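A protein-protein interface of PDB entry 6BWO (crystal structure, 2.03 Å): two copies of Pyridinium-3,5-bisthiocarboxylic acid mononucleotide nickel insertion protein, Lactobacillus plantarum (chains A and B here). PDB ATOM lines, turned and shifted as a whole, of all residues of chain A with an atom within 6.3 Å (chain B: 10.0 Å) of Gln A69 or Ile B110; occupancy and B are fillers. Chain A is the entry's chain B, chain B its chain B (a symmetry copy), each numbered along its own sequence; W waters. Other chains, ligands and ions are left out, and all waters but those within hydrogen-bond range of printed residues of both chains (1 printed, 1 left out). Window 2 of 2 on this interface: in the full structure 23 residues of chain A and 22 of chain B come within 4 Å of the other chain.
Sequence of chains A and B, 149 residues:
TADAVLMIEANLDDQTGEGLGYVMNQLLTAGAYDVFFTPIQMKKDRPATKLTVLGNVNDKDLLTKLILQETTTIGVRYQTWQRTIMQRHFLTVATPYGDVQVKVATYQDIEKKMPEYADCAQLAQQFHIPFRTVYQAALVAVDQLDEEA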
ATOM      1  N   THR A  64      10.790 -21.341 -27.235  1.00  0.00           N
ATOM      2  CA  THR A  64      10.551 -20.078 -27.926  1.00  0.00           C
ATOM      3  C   THR A  64       9.529 -19.247 -27.170  1.00  0.00           C
ATOM      4  O   THR A  64       9.767 -18.076 -26.854  1.00  0.00           O
ATOM      5  CB  THR A  64      10.059 -20.335 -29.350  1.00  0.00           C
ATOM      6  OG1 THR A  64      11.043 -21.076 -30.068  1.00  0.00           O
ATOM      7  CG2 THR A  64       9.819 -19.053 -30.061  1.00  0.00           C
ATOM      8  N   LYS A  65       8.381 -19.857 -26.872  1.00  0.00           N
ATOM      9  CA  LYS A  65       7.282 -19.165 -26.216  1.00  0.00           C
ATOM     10  C   LYS A  65       7.684 -18.639 -24.849  1.00  0.00           C
ATOM     11  O   LYS A  65       7.296 -17.534 -24.465  1.00  0.00           O
ATOM     12  CB  LYS A  65       6.092 -20.117 -26.097  1.00  0.00           C
ATOM     13  CG  LYS A  65       5.126 -19.784 -24.973  1.00  0.00           C
ATOM     14  CD  LYS A  65       4.560 -21.040 -24.307  1.00  0.00           C
ATOM     15  CE  LYS A  65       3.919 -20.680 -22.982  1.00  0.00           C
ATOM     16  NZ  LYS A  65       3.128 -19.408 -23.113  1.00  0.00           N
ATOM     17  N   LEU A  66       8.468 -19.410 -24.101  1.00  0.00           N
ATOM     18  CA  LEU A  66       8.959 -18.923 -22.822  1.00  0.00           C
ATOM     19  C   LEU A  66       9.786 -17.663 -23.009  1.00  0.00           C
ATOM     20  O   LEU A  66       9.616 -16.677 -22.287  1.00  0.00           O
ATOM     21  CB  LEU A  66       9.781 -20.004 -22.138  1.00  0.00           C
ATOM     22  CG  LEU A  66       9.066 -20.785 -21.056  1.00  0.00           C
ATOM     23  CD1 LEU A  66       7.735 -21.228 -21.556  1.00  0.00           C
ATOM     24  CD2 LEU A  66       9.896 -21.974 -20.686  1.00  0.00           C
ATOM     25  N   ILE A  67      10.694 -17.679 -23.980  1.00  0.00           N
ATOM     26  CA  ILE A  67      11.561 -16.528 -24.207  1.00  0.00           C
ATOM     27  C   ILE A  67      10.744 -15.319 -24.631  1.00  0.00           C
ATOM     28  O   ILE A  67      10.979 -14.193 -24.180  1.00  0.00           O
ATOM     29  CB  ILE A  67      12.628 -16.876 -25.263  1.00  0.00           C
ATOM     30  CG1 ILE A  67      13.590 -17.943 -24.757  1.00  0.00           C
ATOM     31  CG2 ILE A  67      13.386 -15.629 -25.674  1.00  0.00           C
ATOM     32  CD1 ILE A  67      14.468 -18.526 -25.836  1.00  0.00           C
ATOM     33  N   LEU A  68       9.784 -15.530 -25.527  1.00  0.00           N
ATOM     34  CA  LEU A  68       8.994 -14.421 -26.036  1.00  0.00           C
ATOM     35  C   LEU A  68       8.006 -13.915 -24.995  1.00  0.00           C
ATOM     36  O   LEU A  68       7.667 -12.731 -24.988  1.00  0.00           O
ATOM     37  CB  LEU A  68       8.281 -14.859 -27.312  1.00  0.00           C
ATOM     38  CG  LEU A  68       9.254 -15.159 -28.447  1.00  0.00           C
ATOM     39  CD1 LEU A  68       8.539 -15.692 -29.630  1.00  0.00           C
ATOM     40  CD2 LEU A  68       9.939 -13.889 -28.823  1.00  0.00           C
ATOM     41  N   GLN A  69       7.572 -14.784 -24.087  1.00  0.00           N
ATOM     42  CA  GLN A  69       6.617 -14.398 -23.054  1.00  0.00           C
ATOM     43  C   GLN A  69       7.298 -13.685 -21.900  1.00  0.00           C
ATOM     44  O   GLN A  69       6.722 -12.779 -21.286  1.00  0.00           O
ATOM     45  CB  GLN A  69       5.895 -15.638 -22.532  1.00  0.00           C
ATOM     46  CG  GLN A  69       4.703 -15.356 -21.657  1.00  0.00           C
ATOM     47  CD  GLN A  69       4.419 -16.491 -20.689  1.00  0.00           C
ATOM     48  OE1 GLN A  69       5.289 -16.915 -19.935  1.00  0.00           O
ATOM     49  NE2 GLN A  69       3.196 -17.000 -20.722  1.00  0.00           N
ATOM     50  N   GLU A  70       8.507 -14.106 -21.574  1.00  0.00           N
ATOM     51  CA  GLU A  70       9.139 -13.672 -20.347  1.00  0.00           C
ATOM     52  C   GLU A  70      10.164 -12.574 -20.555  1.00  0.00           C
ATOM     53  O   GLU A  70      10.426 -11.804 -19.629  1.00  0.00           O
ATOM     54  CB  GLU A  70       9.797 -14.875 -19.675  1.00  0.00           C
ATOM     55  CG  GLU A  70       8.815 -15.939 -19.284  1.00  0.00           C
ATOM     56  CD  GLU A  70       7.954 -15.525 -18.121  1.00  0.00           C
ATOM     57  OE1 GLU A  70       8.327 -14.562 -17.422  1.00  0.00           O
ATOM     58  OE2 GLU A  70       6.911 -16.175 -17.896  1.00  0.00           O
ATOM     59  N   THR A  71      10.754 -12.480 -21.733  1.00  0.00           N
ATOM     60  CA  THR A  71      11.697 -11.418 -22.033  1.00  0.00           C
ATOM     61  C   THR A  71      11.073 -10.400 -22.964  1.00  0.00           C
ATOM     62  O   THR A  71       9.939 -10.533 -23.417  1.00  0.00           O
ATOM     63  CB  THR A  71      12.972 -11.961 -22.658  1.00  0.00           C
ATOM     64  OG1 THR A  71      12.714 -12.242 -24.035  1.00  0.00           O
ATOM     65  CG2 THR A  71      13.403 -13.206 -21.947  1.00  0.00           C
ATOM     66  N   THR B  84      11.642 -16.784 -35.299  1.00  0.00           N
ATOM     67  CA  THR B  84      10.251 -16.778 -34.869  1.00  0.00           C
ATOM     68  C   THR B  84      10.007 -15.422 -34.233  1.00  0.00           C
ATOM     69  O   THR B  84      10.564 -15.115 -33.175  1.00  0.00           O
ATOM     70  CB  THR B  84       9.931 -17.906 -33.898  1.00  0.00           C
ATOM     71  OG1 THR B  84       9.994 -19.161 -34.577  1.00  0.00           O
ATOM     72  CG2 THR B  84       8.531 -17.722 -33.368  1.00  0.00           C
ATOM     73  N   ILE B  85       9.175 -14.617 -34.875  1.00  0.00           N
ATOM     74  CA  ILE B  85       8.993 -13.218 -34.521  1.00  0.00           C
ATOM     75  C   ILE B  85       7.562 -12.992 -34.059  1.00  0.00           C
ATOM     76  O   ILE B  85       6.631 -13.634 -34.561  1.00  0.00           O
ATOM     77  CB  ILE B  85       9.331 -12.317 -35.726  1.00  0.00           C
ATOM     78  CG1 ILE B  85      10.658 -12.741 -36.336  1.00  0.00           C
ATOM     79  CG2 ILE B  85       9.339 -10.833 -35.346  1.00  0.00           C
ATOM     80  CD1 ILE B  85      10.788 -12.363 -37.793  1.00  0.00           C
ATOM     81  N   MET B  86       7.395 -12.111 -33.074  1.00  0.00           N
ATOM     82  CA  MET B  86       6.077 -11.668 -32.654  1.00  0.00           C
ATOM     83  C   MET B  86       5.556 -10.564 -33.577  1.00  0.00           C
ATOM     84  O   MET B  86       6.325  -9.834 -34.211  1.00  0.00           O
ATOM     85  CB  MET B  86       6.110 -11.168 -31.213  1.00  0.00           C
ATOM     86  CG  MET B  86       6.815 -12.061 -30.218  1.00  0.00           C
ATOM     87  SD  MET B  86       7.032 -11.238 -28.642  1.00  0.00           S
ATOM     88  CE  MET B  86       5.777 -12.055 -27.687  1.00  0.00           C
ATOM     89  N   GLN B  87       4.231 -10.441 -33.645  1.00  0.00           N
ATOM     90  CA  GLN B  87       3.611  -9.393 -34.442  1.00  0.00           C
ATOM     91  C   GLN B  87       3.572  -8.105 -33.639  1.00  0.00           C
ATOM     92  O   GLN B  87       3.138  -8.108 -32.487  1.00  0.00           O
ATOM     93  CB  GLN B  87       2.209  -9.813 -34.860  1.00  0.00           C
ATOM     94  CG  GLN B  87       2.218 -10.906 -35.904  1.00  0.00           C
ATOM     95  CD  GLN B  87       1.328 -10.598 -37.079  1.00  0.00           C
ATOM     96  OE1 GLN B  87       1.283  -9.463 -37.559  1.00  0.00           O
ATOM     97  NE2 GLN B  87       0.633 -11.615 -37.575  1.00  0.00           N
ATOM     98  N   ARG B  88       3.998  -7.002 -34.244  1.00  0.00           N
ATOM     99  CA  ARG B  88       4.090  -5.729 -33.541  1.00  0.00           C
ATOM    100  C   ARG B  88       2.898  -4.852 -33.863  1.00  0.00           C
ATOM    101  O   ARG B  88       2.300  -4.948 -34.934  1.00  0.00           O
ATOM    102  CB  ARG B  88       5.355  -4.937 -33.907  1.00  0.00           C
ATOM    103  CG  ARG B  88       6.680  -5.665 -33.869  1.00  0.00           C
ATOM    104  CD  ARG B  88       7.780  -4.868 -34.619  1.00  0.00           C
ATOM    105  NE  ARG B  88       8.899  -4.435 -33.762  1.00  0.00           N
ATOM    106  CZ  ARG B  88      10.158  -4.874 -33.852  1.00  0.00           C
ATOM    107  NH1 ARG B  88      10.494  -5.769 -34.766  1.00  0.00           N
ATOM    108  NH2 ARG B  88      11.086  -4.411 -33.030  1.00  0.00           N
ATOM    109  N   HIS B  89       2.534  -4.017 -32.901  1.00  0.00           N
ATOM    110  CA  HIS B  89       1.759  -2.828 -33.200  1.00  0.00           C
ATOM    111  C   HIS B  89       2.061  -1.804 -32.117  1.00  0.00           C
ATOM    112  O   HIS B  89       2.585  -2.138 -31.052  1.00  0.00           O
ATOM    113  CB  HIS B  89       0.254  -3.109 -33.320  1.00  0.00           C
ATOM    114  CG  HIS B  89      -0.416  -3.474 -32.035  1.00  0.00           C
ATOM    115  ND1 HIS B  89      -0.459  -4.764 -31.557  1.00  0.00           N
ATOM    116  CD2 HIS B  89      -1.115  -2.725 -31.153  1.00  0.00           C
ATOM    117  CE1 HIS B  89      -1.140  -4.791 -30.427  1.00  0.00           C
ATOM    118  NE2 HIS B  89      -1.552  -3.565 -30.162  1.00  0.00           N
ATOM    119  N   VAL B 104       3.397  -2.773 -28.583  1.00  0.00           N
ATOM    120  CA  VAL B 104       2.662  -3.904 -28.045  1.00  0.00           C
ATOM    121  C   VAL B 104       2.998  -5.105 -28.901  1.00  0.00           C
ATOM    122  O   VAL B 104       2.770  -5.091 -30.115  1.00  0.00           O
ATOM    123  CB  VAL B 104       1.156  -3.639 -28.037  1.00  0.00           C
ATOM    124  CG1 VAL B 104       0.440  -4.781 -27.350  1.00  0.00           C
ATOM    125  CG2 VAL B 104       0.876  -2.325 -27.345  1.00  0.00           C
ATOM    126  N   ALA B 105       3.560  -6.131 -28.282  1.00  0.00           N
ATOM    127  CA  ALA B 105       3.998  -7.317 -28.996  1.00  0.00           C
ATOM    128  C   ALA B 105       3.113  -8.489 -28.613  1.00  0.00           C
ATOM    129  O   ALA B 105       2.854  -8.728 -27.430  1.00  0.00           O
ATOM    130  CB  ALA B 105       5.463  -7.630 -28.700  1.00  0.00           C
ATOM    131  N   THR B 106       2.663  -9.219 -29.619  1.00  0.00           N
ATOM    132  CA  THR B 106       1.776 -10.344 -29.427  1.00  0.00           C
ATOM    133  C   THR B 106       2.344 -11.549 -30.153  1.00  0.00           C
ATOM    134  O   THR B 106       3.008 -11.424 -31.183  1.00  0.00           O
ATOM    135  CB  THR B 106       0.368 -10.032 -29.931  1.00  0.00           C
ATOM    136  OG1 THR B 106       0.438  -9.562 -31.283  1.00  0.00           O
ATOM    137  CG2 THR B 106      -0.256  -8.961 -29.080  1.00  0.00           C
ATOM    138  N   TYR B 107       2.094 -12.724 -29.602  1.00  0.00           N
ATOM    139  CA  TYR B 107       2.419 -13.945 -30.323  1.00  0.00           C
ATOM    140  C   TYR B 107       1.567 -15.054 -29.739  1.00  0.00           C
ATOM    141  O   TYR B 107       1.628 -15.318 -28.530  1.00  0.00           O
ATOM    142  CB  TYR B 107       3.910 -14.252 -30.218  1.00  0.00           C
ATOM    143  CG  TYR B 107       4.354 -15.522 -30.886  1.00  0.00           C
ATOM    144  CD1 TYR B 107       4.523 -15.581 -32.254  1.00  0.00           C
ATOM    145  CD2 TYR B 107       4.648 -16.646 -30.144  1.00  0.00           C
ATOM    146  CE1 TYR B 107       4.940 -16.738 -32.860  1.00  0.00           C
ATOM    147  CE2 TYR B 107       5.062 -17.800 -30.739  1.00  0.00           C
ATOM    148  CZ  TYR B 107       5.209 -17.844 -32.093  1.00  0.00           C
ATOM    149  OH  TYR B 107       5.633 -19.012 -32.672  1.00  0.00           O
ATOM    150  N   GLN B 108       0.744 -15.663 -30.583  1.00  0.00           N
ATOM    151  CA  GLN B 108      -0.216 -16.639 -30.105  1.00  0.00           C
ATOM    152  C   GLN B 108      -1.024 -16.011 -28.979  1.00  0.00           C
ATOM    153  O   GLN B 108      -1.887 -15.157 -29.216  1.00  0.00           O
ATOM    154  CB  GLN B 108       0.505 -17.906 -29.643  1.00  0.00           C
ATOM    155  CG  GLN B 108       1.611 -18.327 -30.600  1.00  0.00           C
ATOM    156  CD  GLN B 108       1.947 -19.795 -30.535  1.00  0.00           C
ATOM    157  OE1 GLN B 108       1.760 -20.446 -29.509  1.00  0.00           O
ATOM    158  NE2 GLN B 108       2.495 -20.316 -31.624  1.00  0.00           N
ATOM    159  N   ASP B 109      -0.711 -16.401 -27.747  1.00  0.00           N
ATOM    160  CA  ASP B 109      -1.438 -15.972 -26.564  1.00  0.00           C
ATOM    161  C   ASP B 109      -0.600 -15.096 -25.645  1.00  0.00           C
ATOM    162  O   ASP B 109      -0.908 -14.980 -24.456  1.00  0.00           O
ATOM    163  CB  ASP B 109      -1.969 -17.200 -25.837  1.00  0.00           C
ATOM    164  CG  ASP B 109      -0.883 -18.197 -25.547  1.00  0.00           C
ATOM    165  OD1 ASP B 109      -0.099 -18.488 -26.473  1.00  0.00           O
ATOM    166  OD2 ASP B 109      -0.825 -18.717 -24.416  1.00  0.00           O
ATOM    167  N   ILE B 110       0.472 -14.508 -26.164  1.00  0.00           N
ATOM    168  CA  ILE B 110       1.336 -13.598 -25.421  1.00  0.00           C
ATOM    169  C   ILE B 110       1.048 -12.167 -25.850  1.00  0.00           C
ATOM    170  O   ILE B 110       0.948 -11.892 -27.046  1.00  0.00           O
ATOM    171  CB  ILE B 110       2.812 -13.934 -25.664  1.00  0.00           C
ATOM    172  CG1 ILE B 110       3.120 -15.364 -25.208  1.00  0.00           C
ATOM    173  CG2 ILE B 110       3.679 -12.897 -24.994  1.00  0.00           C
ATOM    174  CD1 ILE B 110       4.419 -15.933 -25.742  1.00  0.00           C
ATOM    175  N   GLU B 111       0.933 -11.249 -24.890  1.00  0.00           N
ATOM    176  CA  GLU B 111       0.762  -9.833 -25.202  1.00  0.00           C
ATOM    177  C   GLU B 111       1.583  -9.018 -24.213  1.00  0.00           C
ATOM    178  O   GLU B 111       1.336  -9.087 -23.006  1.00  0.00           O
ATOM    179  CB  GLU B 111      -0.714  -9.422 -25.140  1.00  0.00           C
ATOM    180  CG  GLU B 111      -0.991  -8.101 -25.826  1.00  0.00           C
ATOM    181  CD  GLU B 111      -2.009  -7.250 -25.117  1.00  0.00           C
ATOM    182  OE1 GLU B 111      -2.221  -7.446 -23.905  1.00  0.00           O
ATOM    183  OE2 GLU B 111      -2.595  -6.371 -25.776  1.00  0.00           O
ATOM    184  N   LYS B 112       2.544  -8.234 -24.711  1.00  0.00           N
ATOM    185  CA  LYS B 112       3.392  -7.433 -23.835  1.00  0.00           C
ATOM    186  C   LYS B 112       3.657  -6.080 -24.469  1.00  0.00           C
ATOM    187  O   LYS B 112       3.650  -5.934 -25.689  1.00  0.00           O
ATOM    188  CB  LYS B 112       4.734  -8.125 -23.503  1.00  0.00           C
ATOM    189  CG  LYS B 112       5.697  -8.262 -24.671  1.00  0.00           C
ATOM    190  CD  LYS B 112       6.986  -9.005 -24.279  1.00  0.00           C
ATOM    191  CE  LYS B 112       7.834  -9.254 -25.515  1.00  0.00           C
ATOM    192  NZ  LYS B 112       8.861 -10.318 -25.353  1.00  0.00           N
ATOM    193  N   LYS B 113       3.907  -5.090 -23.617  1.00  0.00           N
ATOM    194  CA  LYS B 113       3.986  -3.696 -24.033  1.00  0.00           C
ATOM    195  C   LYS B 113       5.293  -3.084 -23.553  1.00  0.00           C
ATOM    196  O   LYS B 113       5.598  -3.130 -22.360  1.00  0.00           O
ATOM    197  CB  LYS B 113       2.765  -2.927 -23.515  1.00  0.00           C
ATOM    198  CG  LYS B 113       1.458  -3.620 -23.911  1.00  0.00           C
ATOM    199  CD  LYS B 113       0.383  -3.582 -22.834  1.00  0.00           C
ATOM    200  CE  LYS B 113       0.860  -4.220 -21.535  1.00  0.00           C
ATOM    201  NZ  LYS B 113       1.293  -5.642 -21.691  1.00  0.00           N
ATOM    202  N   MET B 114       6.064  -2.528 -24.486  1.00  0.00           N
ATOM    203  CA  MET B 114       7.365  -1.920 -24.201  1.00  0.00           C
ATOM    204  C   MET B 114       7.340  -0.440 -24.524  1.00  0.00           C
ATOM    205  O   MET B 114       7.301  -0.083 -25.714  1.00  0.00           O
ATOM    206  CB  MET B 114       8.455  -2.590 -25.032  1.00  0.00           C
ATOM    207  CG  MET B 114       9.128  -3.728 -24.342  1.00  0.00           C
ATOM    208  SD  MET B 114       8.175  -5.173 -24.698  1.00  0.00           S
ATOM    209  CE  MET B 114       8.184  -5.130 -26.483  1.00  0.00           C
HETATM  210  O   HOH W   1      10.537 -20.788 -32.685  1.00  0.00           O
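Printed residues of chain B within 4 Å of Gln A69: Ile B110 (3.5 Å). Printed residues of chain A within 4 Å of Ile B110: Lys A65, Leu A68 and Gln A69. Of the printed residues of chain B, Lys A65 touches Ile B110 (3.5 Å). No residue of chain B comes within 4 Å of Glu A70. Printed residues of chain B within 4 Å of Thr A64: Thr B84 (3.8 Å). Of the printed residues of chain B, Thr A71 touches Lys B112. Printed residues of chain A within 4 Å of Met B86: Leu A68 (3.4 Å). Printed residues of chain A within 4 Å of Lys B112: Leu A68 (2.7 Å) and Thr A71 (2.2 Å). Of the printed residues of chain B, Leu A68 touches Met B86, Ile B110 and Lys B112. The nearest printed residue of chain A that does not touch Ile B110 is Leu A66 (5.6 Å).
Of the 17 printed residues of chain B, 4 touch a printed residue of chain A. Hydrophobic or aromatic side chains of chain B that line the printed part of chain A: Met B86 and Ile B110. Hydrophobic or aromatic side chains of chain A that line the printed part of chain B: Leu A68. Along chain A the printed residues that touch a printed residue of chain B span positions 64 to 71.
Among the printed residues, pairs that only touch across the chains: Leu A68 with Met B86, Lys A65 with Ile B110, Gln A69 with Ile B110, Thr A64 with Thr B84 and Leu A68 with Ile B110.
The backbone carbonyl oxygen (O) of Thr A71 sits close to the side-chain amino group (NZ) of Lys B112 (2.2 Å). The side-chain amino group (NZ) of Lys B112 sits at hydrogen-bond distance from the backbone carbonyl oxygen (O) of Leu A68 (2.7 Å).
Water W1 bridges OG1 of Thr B84 (2.6 Å) and OG1 of Thr A64 (2.7 Å).
No position is printed for both chains.
O of Ile A67 lies within hydrogen-bond range of OG1 of Thr A71. The side-chain amino group (NZ) of Lys A65 lies close to the side-chain amide nitrogen (NE2) of Gln A69, at 3.4 Å. The side-chain carboxylate of Glu A70 lies close to the side-chain amide oxygen of Gln A69 (2.7 Å). The backbone carbonyl oxygen (O) of Lys B112 sits at hydrogen-bond distance from the backbone NH (N) of Ala B105.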
